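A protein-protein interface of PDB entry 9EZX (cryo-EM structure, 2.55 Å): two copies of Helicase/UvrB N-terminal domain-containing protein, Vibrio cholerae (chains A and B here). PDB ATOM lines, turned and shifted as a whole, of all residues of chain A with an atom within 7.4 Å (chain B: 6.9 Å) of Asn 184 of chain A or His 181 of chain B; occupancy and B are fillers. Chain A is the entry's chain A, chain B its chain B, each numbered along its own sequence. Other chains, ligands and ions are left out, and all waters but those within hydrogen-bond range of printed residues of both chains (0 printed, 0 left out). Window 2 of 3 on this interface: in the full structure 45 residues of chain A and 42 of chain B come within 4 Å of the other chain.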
ATOM      1  N   LEU A 178      26.489  27.942 -15.439  1.00  0.00           N
ATOM      2  CA  LEU A 178      25.290  27.382 -16.055  1.00  0.00           C
ATOM      3  C   LEU A 178      25.648  26.443 -17.197  1.00  0.00           C
ATOM      4  O   LEU A 178      24.908  25.493 -17.476  1.00  0.00           O
ATOM      5  CB  LEU A 178      24.374  28.493 -16.570  1.00  0.00           C
ATOM      6  CG  LEU A 178      23.432  29.151 -15.562  1.00  0.00           C
ATOM      7  CD1 LEU A 178      22.951  30.499 -16.077  1.00  0.00           C
ATOM      8  CD2 LEU A 178      22.253  28.242 -15.260  1.00  0.00           C
ATOM      9  N   ARG A 180      27.792  24.171 -17.197  1.00  0.00           N
ATOM     10  CA  ARG A 180      27.992  22.832 -16.658  1.00  0.00           C
ATOM     11  C   ARG A 180      26.685  22.075 -16.482  1.00  0.00           C
ATOM     12  O   ARG A 180      26.686  20.841 -16.537  1.00  0.00           O
ATOM     13  CB  ARG A 180      28.710  22.908 -15.310  1.00  0.00           C
ATOM     14  CG  ARG A 180      30.189  23.220 -15.410  1.00  0.00           C
ATOM     15  CD  ARG A 180      30.407  24.628 -15.926  1.00  0.00           C
ATOM     16  NE  ARG A 180      31.812  25.003 -15.909  1.00  0.00           N
ATOM     17  CZ  ARG A 180      32.398  25.684 -14.933  1.00  0.00           C
ATOM     18  NH1 ARG A 180      31.732  26.060 -13.852  1.00  0.00           N
ATOM     19  NH2 ARG A 180      33.687  25.988 -15.041  1.00  0.00           N
ATOM     20  N   HIS A 181      25.577  22.790 -16.290  1.00  0.00           N
ATOM     21  CA  HIS A 181      24.261  22.179 -16.156  1.00  0.00           C
ATOM     22  C   HIS A 181      23.406  22.429 -17.386  1.00  0.00           C
ATOM     23  O   HIS A 181      22.176  22.350 -17.305  1.00  0.00           O
ATOM     24  CB  HIS A 181      23.537  22.700 -14.910  1.00  0.00           C
ATOM     25  CG  HIS A 181      24.256  22.430 -13.623  1.00  0.00           C
ATOM     26  ND1 HIS A 181      24.401  21.165 -13.094  1.00  0.00           N
ATOM     27  CD2 HIS A 181      24.872  23.270 -12.759  1.00  0.00           C
ATOM     28  CE1 HIS A 181      25.077  21.238 -11.962  1.00  0.00           C
ATOM     29  NE2 HIS A 181      25.375  22.504 -11.735  1.00  0.00           N
ATOM     30  N   ALA A 182      24.032  22.744 -18.519  1.00  0.00           N
ATOM     31  CA  ALA A 182      23.307  23.035 -19.744  1.00  0.00           C
ATOM     32  C   ALA A 182      22.505  21.846 -20.254  1.00  0.00           C
ATOM     33  O   ALA A 182      21.573  22.046 -21.042  1.00  0.00           O
ATOM     34  CB  ALA A 182      24.307  23.502 -20.805  1.00  0.00           C
ATOM     35  N   SER A 183      22.824  20.623 -19.815  1.00  0.00           N
ATOM     36  CA  SER A 183      22.113  19.453 -20.320  1.00  0.00           C
ATOM     37  C   SER A 183      20.613  19.571 -20.092  1.00  0.00           C
ATOM     38  O   SER A 183      19.819  19.109 -20.920  1.00  0.00           O
ATOM     39  CB  SER A 183      22.640  18.178 -19.655  1.00  0.00           C
ATOM     40  OG  SER A 183      22.497  18.237 -18.247  1.00  0.00           O
ATOM     41  N   ASN A 184      20.210  20.190 -18.995  1.00  0.00           N
ATOM     42  CA  ASN A 184      18.799  20.267 -18.656  1.00  0.00           C
ATOM     43  C   ASN A 184      18.083  21.247 -19.583  1.00  0.00           C
ATOM     44  O   ASN A 184      18.648  22.291 -19.924  1.00  0.00           O
ATOM     45  CB  ASN A 184      18.628  20.691 -17.207  1.00  0.00           C
ATOM     46  CG  ASN A 184      17.209  21.067 -16.886  1.00  0.00           C
ATOM     47  OD1 ASN A 184      16.726  22.110 -17.317  1.00  0.00           O
ATOM     48  ND2 ASN A 184      16.521  20.211 -16.142  1.00  0.00           N
ATOM     49  N   PRO A 185      16.846  20.953 -20.003  1.00  0.00           N
ATOM     50  CA  PRO A 185      16.173  21.847 -20.967  1.00  0.00           C
ATOM     51  C   PRO A 185      15.902  23.248 -20.443  1.00  0.00           C
ATOM     52  O   PRO A 185      16.293  24.234 -21.082  1.00  0.00           O
ATOM     53  CB  PRO A 185      14.869  21.096 -21.274  1.00  0.00           C
ATOM     54  CG  PRO A 185      15.158  19.677 -20.967  1.00  0.00           C
ATOM     55  CD  PRO A 185      16.110  19.691 -19.818  1.00  0.00           C
ATOM     56  N   GLU A 186      15.205  23.372 -19.310  1.00  0.00           N
ATOM     57  CA  GLU A 186      14.908  24.704 -18.790  1.00  0.00           C
ATOM     58  C   GLU A 186      16.187  25.464 -18.469  1.00  0.00           C
ATOM     59  O   GLU A 186      16.288  26.668 -18.749  1.00  0.00           O
ATOM     60  CB  GLU A 186      14.003  24.615 -17.558  1.00  0.00           C
ATOM     61  CG  GLU A 186      14.476  23.671 -16.461  1.00  0.00           C
ATOM     62  CD  GLU A 186      14.002  22.245 -16.669  1.00  0.00           C
ATOM     63  OE1 GLU A 186      13.507  21.936 -17.774  1.00  0.00           O
ATOM     64  OE2 GLU A 186      14.129  21.432 -15.730  1.00  0.00           O
ATOM     65  N   VAL A 187      17.174  24.778 -17.892  1.00  0.00           N
ATOM     66  CA  VAL A 187      18.480  25.391 -17.698  1.00  0.00           C
ATOM     67  C   VAL A 187      19.061  25.819 -19.038  1.00  0.00           C
ATOM     68  O   VAL A 187      19.697  26.872 -19.141  1.00  0.00           O
ATOM     69  CB  VAL A 187      19.416  24.423 -16.953  1.00  0.00           C
ATOM     70  CG1 VAL A 187      20.821  25.011 -16.850  1.00  0.00           C
ATOM     71  CG2 VAL A 187      18.839  24.090 -15.582  1.00  0.00           C
ATOM     72  N   LYS A 188      18.850  25.018 -20.088  1.00  0.00           N
ATOM     73  CA  LYS A 188      19.366  25.380 -21.406  1.00  0.00           C
ATOM     74  C   LYS A 188      18.748  26.677 -21.914  1.00  0.00           C
ATOM     75  O   LYS A 188      19.461  27.550 -22.423  1.00  0.00           O
ATOM     76  CB  LYS A 188      19.130  24.230 -22.390  1.00  0.00           C
ATOM     77  CG  LYS A 188      19.688  24.438 -23.810  1.00  0.00           C
ATOM     78  CD  LYS A 188      19.490  23.261 -24.777  1.00  0.00           C
ATOM     79  CE  LYS A 188      20.026  23.496 -26.178  1.00  0.00           C
ATOM     80  NZ  LYS A 188      19.798  22.314 -27.057  1.00  0.00           N
ATOM     81  N   ILE A 189      17.429  26.833 -21.785  1.00  0.00           N
ATOM     82  CA  ILE A 189      16.792  28.041 -22.316  1.00  0.00           C
ATOM     83  C   ILE A 189      17.207  29.255 -21.490  1.00  0.00           C
ATOM     84  O   ILE A 189      17.478  30.337 -22.032  1.00  0.00           O
ATOM     85  CB  ILE A 189      15.258  27.887 -22.381  1.00  0.00           C
ATOM     86  CG1 ILE A 189      14.595  29.261 -22.556  1.00  0.00           C
ATOM     87  CG2 ILE A 189      14.714  27.230 -21.133  1.00  0.00           C
ATOM     88  CD1 ILE A 189      13.092  29.217 -22.753  1.00  0.00           C
ATOM     89  N   SER A 190      17.263  29.096 -20.164  1.00  0.00           N
ATOM     90  CA  SER A 190      17.733  30.195 -19.326  1.00  0.00           C
ATOM     91  C   SER A 190      19.160  30.586 -19.689  1.00  0.00           C
ATOM     92  O   SER A 190      19.491  31.777 -19.760  1.00  0.00           O
ATOM     93  CB  SER A 190      17.647  29.806 -17.851  1.00  0.00           C
ATOM     94  OG  SER A 190      18.060  28.466 -17.654  1.00  0.00           O
ATOM     95  N   LEU A 191      20.019  29.592 -19.920  1.00  0.00           N
ATOM     96  CA  LEU A 191      21.398  29.870 -20.294  1.00  0.00           C
ATOM     97  C   LEU A 191      21.467  30.581 -21.635  1.00  0.00           C
ATOM     98  O   LEU A 191      22.299  31.470 -21.826  1.00  0.00           O
ATOM     99  CB  LEU A 191      22.198  28.569 -20.335  1.00  0.00           C
ATOM    100  CG  LEU A 191      23.622  28.672 -20.877  1.00  0.00           C
ATOM    101  CD1 LEU A 191      24.409  29.757 -20.158  1.00  0.00           C
ATOM    102  CD2 LEU A 191      24.326  27.331 -20.763  1.00  0.00           C
ATOM    103  N   SER B 176      10.481  29.009 -13.281  1.00  0.00           N
ATOM    104  CA  SER B 176       9.919  27.837 -12.562  1.00  0.00           C
ATOM    105  C   SER B 176      10.910  26.686 -12.704  1.00  0.00           C
ATOM    106  O   SER B 176      11.116  25.959 -11.715  1.00  0.00           O
ATOM    107  CB  SER B 176       8.559  27.472 -13.092  1.00  0.00           C
ATOM    108  OG  SER B 176       7.669  28.575 -13.004  1.00  0.00           O
ATOM    109  N   GLY B 177      11.484  26.517 -13.895  1.00  0.00           N
ATOM    110  CA  GLY B 177      12.494  25.478 -14.156  1.00  0.00           C
ATOM    111  C   GLY B 177      13.774  25.712 -13.374  1.00  0.00           C
ATOM    112  O   GLY B 177      14.318  24.728 -12.847  1.00  0.00           O
ATOM    113  N   LEU B 178      14.242  26.960 -13.288  1.00  0.00           N
ATOM    114  CA  LEU B 178      15.488  27.331 -12.558  1.00  0.00           C
ATOM    115  C   LEU B 178      15.312  27.011 -11.073  1.00  0.00           C
ATOM    116  O   LEU B 178      16.311  26.614 -10.445  1.00  0.00           O
ATOM    117  CB  LEU B 178      15.794  28.819 -12.765  1.00  0.00           C
ATOM    118  CG  LEU B 178      16.581  29.171 -14.029  1.00  0.00           C
ATOM    119  CD1 LEU B 178      16.226  30.567 -14.529  1.00  0.00           C
ATOM    120  CD2 LEU B 178      18.080  29.057 -13.783  1.00  0.00           C
ATOM    121  N   ARG B 179      14.105  27.190 -10.528  1.00  0.00           N
ATOM    122  CA  ARG B 179      13.804  26.936  -9.092  1.00  0.00           C
ATOM    123  C   ARG B 179      14.056  25.462  -8.760  1.00  0.00           C
ATOM    124  O   ARG B 179      14.384  25.177  -7.597  1.00  0.00           O
ATOM    125  CB  ARG B 179      12.367  27.341  -8.751  1.00  0.00           C
ATOM    126  CG  ARG B 179      12.188  28.841  -8.573  1.00  0.00           C
ATOM    127  CD  ARG B 179      10.738  29.264  -8.461  1.00  0.00           C
ATOM    128  NE  ARG B 179      10.567  30.684  -8.742  1.00  0.00           N
ATOM    129  CZ  ARG B 179       9.436  31.377  -8.602  1.00  0.00           C
ATOM    130  NH1 ARG B 179       8.322  30.807  -8.168  1.00  0.00           N
ATOM    131  NH2 ARG B 179       9.428  32.663  -8.900  1.00  0.00           N
ATOM    132  N   ARG B 180      13.873  24.554  -9.720  1.00  0.00           N
ATOM    133  CA  ARG B 180      14.126  23.100  -9.516  1.00  0.00           C
ATOM    134  C   ARG B 180      15.611  22.905  -9.190  1.00  0.00           C
ATOM    135  O   ARG B 180      15.898  22.026  -8.355  1.00  0.00           O
ATOM    136  CB  ARG B 180      13.702  22.276 -10.740  1.00  0.00           C
ATOM    137  CG  ARG B 180      12.276  22.502 -11.236  1.00  0.00           C
ATOM    138  CD  ARG B 180      11.235  22.842 -10.180  1.00  0.00           C
ATOM    139  NE  ARG B 180      11.206  21.862  -9.095  1.00  0.00           N
ATOM    140  CZ  ARG B 180      10.850  22.087  -7.824  1.00  0.00           C
ATOM    141  NH1 ARG B 180      10.465  23.283  -7.401  1.00  0.00           N
ATOM    142  NH2 ARG B 180      10.884  21.084  -6.961  1.00  0.00           N
ATOM    143  N   HIS B 181      16.513  23.683  -9.802  1.00  0.00           N
ATOM    144  CA  HIS B 181      17.988  23.594  -9.597  1.00  0.00           C
ATOM    145  C   HIS B 181      18.459  24.731  -8.684  1.00  0.00           C
ATOM    146  O   HIS B 181      19.677  24.996  -8.678  1.00  0.00           O
ATOM    147  CB  HIS B 181      18.706  23.584 -10.952  1.00  0.00           C
ATOM    148  CG  HIS B 181      17.906  22.920 -12.017  1.00  0.00           C
ATOM    149  ND1 HIS B 181      17.824  21.548 -12.132  1.00  0.00           N
ATOM    150  CD2 HIS B 181      17.118  23.433 -12.983  1.00  0.00           C
ATOM    151  CE1 HIS B 181      17.036  21.244 -13.141  1.00  0.00           C
ATOM    152  NE2 HIS B 181      16.591  22.384 -13.678  1.00  0.00           N
ATOM    153  N   ALA B 182      17.560  25.344  -7.909  1.00  0.00           N
ATOM    154  CA  ALA B 182      17.867  26.489  -7.013  1.00  0.00           C
ATOM    155  C   ALA B 182      18.893  26.078  -5.953  1.00  0.00           C
ATOM    156  O   ALA B 182      19.546  26.977  -5.403  1.00  0.00           O
ATOM    157  CB  ALA B 182      16.605  27.000  -6.362  1.00  0.00           C
ATOM    158  N   SER B 183      19.042  24.785  -5.665  1.00  0.00           N
ATOM    159  CA  SER B 183      19.981  24.285  -4.631  1.00  0.00           C
ATOM    160  C   SER B 183      21.398  24.766  -4.962  1.00  0.00           C
ATOM    161  O   SER B 183      22.108  25.165  -4.017  1.00  0.00           O
ATOM    162  CB  SER B 183      19.929  22.784  -4.545  1.00  0.00           C
ATOM    163  OG  SER B 183      20.373  22.196  -5.758  1.00  0.00           O
ATOM    164  N   ASN B 184      21.793  24.753  -6.239  1.00  0.00           N
ATOM    165  CA  ASN B 184      23.128  25.252  -6.670  1.00  0.00           C
ATOM    166  C   ASN B 184      23.191  26.766  -6.404  1.00  0.00           C
ATOM    167  O   ASN B 184      22.244  27.459  -6.827  1.00  0.00           O
ATOM    168  CB  ASN B 184      23.395  24.948  -8.145  1.00  0.00           C
ATOM    169  CG  ASN B 184      24.741  25.454  -8.618  1.00  0.00           C
ATOM    170  OD1 ASN B 184      24.818  26.450  -9.333  1.00  0.00           O
ATOM    171  ND2 ASN B 184      25.809  24.778  -8.227  1.00  0.00           N
ATOM    172  N   PRO B 185      24.234  27.334  -5.749  1.00  0.00           N
ATOM    173  CA  PRO B 185      24.263  28.771  -5.465  1.00  0.00           C
ATOM    174  C   PRO B 185      24.318  29.626  -6.740  1.00  0.00           C
ATOM    175  O   PRO B 185      23.683  30.662  -6.767  1.00  0.00           O
ATOM    176  CB  PRO B 185      25.533  29.004  -4.632  1.00  0.00           C
ATOM    177  CG  PRO B 185      25.961  27.628  -4.174  1.00  0.00           C
ATOM    178  CD  PRO B 185      25.417  26.659  -5.202  1.00  0.00           C
ATOM    179  N   GLU B 186      25.086  29.204  -7.747  1.00  0.00           N
ATOM    180  CA  GLU B 186      25.235  29.969  -9.017  1.00  0.00           C
ATOM    181  C   GLU B 186      23.880  30.032  -9.728  1.00  0.00           C
ATOM    182  O   GLU B 186      23.576  31.093 -10.312  1.00  0.00           O
ATOM    183  CB  GLU B 186      26.308  29.384  -9.939  1.00  0.00           C
ATOM    184  CG  GLU B 186      27.353  30.402 -10.358  1.00  0.00           C
ATOM    185  CD  GLU B 186      28.023  30.094 -11.681  1.00  0.00           C
ATOM    186  OE1 GLU B 186      29.233  29.793 -11.676  1.00  0.00           O
ATOM    187  OE2 GLU B 186      27.326  30.156 -12.711  1.00  0.00           O
ATOM    188  N   VAL B 187      23.097  28.950  -9.686  1.00  0.00           N
ATOM    189  CA  VAL B 187      21.753  28.904 -10.335  1.00  0.00           C
ATOM    190  C   VAL B 187      20.885  29.981  -9.679  1.00  0.00           C
ATOM    191  O   VAL B 187      20.129  30.626 -10.408  1.00  0.00           O
ATOM    192  CB  VAL B 187      21.086  27.516 -10.259  1.00  0.00           C
ATOM    193  CG1 VAL B 187      19.591  27.588 -10.552  1.00  0.00           C
ATOM    194  CG2 VAL B 187      21.755  26.515 -11.191  1.00  0.00           C
ATOM    195  N   LYS B 188      20.997  30.176  -8.360  1.00  0.00           N
ATOM    196  CA  LYS B 188      20.183  31.189  -7.636  1.00  0.00           C
ATOM    197  C   LYS B 188      20.487  32.577  -8.193  1.00  0.00           C
ATOM    198  O   LYS B 188      19.534  33.343  -8.366  1.00  0.00           O
ATOM    199  CB  LYS B 188      20.478  31.252  -6.133  1.00  0.00           C
ATOM    200  CG  LYS B 188      19.874  30.155  -5.271  1.00  0.00           C
ATOM    201  CD  LYS B 188      18.380  29.919  -5.439  1.00  0.00           C
ATOM    202  CE  LYS B 188      17.503  31.156  -5.402  1.00  0.00           C
ATOM    203  NZ  LYS B 188      17.680  31.947  -4.161  1.00  0.00           N
ATOM    204  N   LEU B 191      18.846  32.834 -11.498  1.00  0.00           N
ATOM    205  CA  LEU B 191      17.378  32.744 -11.270  1.00  0.00           C
ATOM    206  C   LEU B 191      16.876  34.098 -10.777  1.00  0.00           C
ATOM    207  O   LEU B 191      15.817  34.514 -11.244  1.00  0.00           O
ATOM    208  CB  LEU B 191      17.081  31.638 -10.246  1.00  0.00           C
ATOM    209  CG  LEU B 191      15.675  31.617  -9.639  1.00  0.00           C
ATOM    210  CD1 LEU B 191      14.588  31.585 -10.707  1.00  0.00           C
ATOM    211  CD2 LEU B 191      15.523  30.437  -8.691  1.00  0.00           C
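The side-chain amide nitrogen (ND2) of Asn 184 of chain A lies close to a ring nitrogen (NE2) of His 181 of chain B (3.3 Å). OE2 of Glu 186 of chain A sits at hydrogen-bond distance from NE2 of His 181 of chain B.
The side-chain amide nitrogen (ND2) of Asn 184 of chain A is in hydrogen-bond range of the side-chain carboxylate (OE2) of Glu 186 of chain A (2.7 Å). OG of Ser 190 of chain A sits at hydrogen-bond distance from O of Val 187 of chain A, at 2.7 Å. The backbone NH (N) of Val 187 of chain A lies within hydrogen-bond range of the side-chain amide oxygen (OD1) of Asn 184 of chain A, at 2.8 Å. The side-chain amide oxygen (OD1) of Asn 184 of chain B sits at hydrogen-bond distance from the backbone NH (N) of Glu 186 of chain B (3.2 Å). The side-chain hydroxyl (OG) of Ser 190 of chain A lies within hydrogen-bond range of the backbone carbonyl oxygen (O) of Glu 186 of chain A, 2.8 Å away. O of Gly 177 of chain B sits close to NE2 of His 181 of chain B (3.4 Å).
Among the printed residues, pairs that only touch across the chains: Val 187 of chain A with His 181 of chain B, Glu 186 of chain A with Gly 177 of chain B, Leu 178 of chain A with Glu 186 of chain B and Ser 190 of chain A with Leu 178 of chain B.
Of the printed residues of chain B, Leu 178 of chain A touches Glu 186 (3.6 Å). Asn 184 of chain A touches just one residue of chain B: His 181 (3.2 Å). Of the printed residues of chain B, Val 187 of chain A touches His 181. Of the printed residues of chain B, Ser 190 of chain A touches Leu 178. Of the printed residues of chain A, Gly 177 of chain B touches Glu 186 (3.5 Å). Printed residues of chain A within 4 Å of Leu 178 of chain B: Ser 190 (3.7 Å). Arg 179 of chain B touches none of the printed residues of chain A. Arg 180 of chain B touches none of the printed residues of chain A. Of chain A, only Asn 184, Glu 186 and Val 187 come within 4 Å of His 181 of chain B. The nearest residue of chain B that does not touch Asn 184 of chain A is Gly 177 of chain B (5.7 Å). The nearest residue of chain A that does not touch His 181 of chain B is His 181 of chain A (6.3 Å). The nearest printed residue of chain B that does not touch Glu 186 of chain A is Leu 178 of chain B (4.6 Å).
Hydrophobic or aromatic side chains of chain B that line the printed part of chain A: Leu 178 and His 181.
Leu 178 of chain A touches Glu 186 of chain B, but with the chains exchanged Glu 186 of chain A does not touch Leu 178 of chain B (4.6 Å). Asn 184 of chain A touches His 181 of chain B, but with the chains exchanged His 181 of chain A does not touch Asn 184 of chain B (4.2 Å). Glu 186 of chain A touches His 181 of chain B, but with the chains exchanged His 181 of chain A does not touch Glu 186 of chain B (6.9 Å). Val 187 of chain A touches His 181 of chain B, but with the chains exchanged His 181 of chain A does not touch Val 187 of chain B (4.8 Å). Positions printed for both chains: 178, 180, 181, 182, 183, 184, 185, 186, 187, 188 and 191. Of the 6 pairs that touch across the chains among the printed residues, none has its exchanged pair printed and touching as well.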
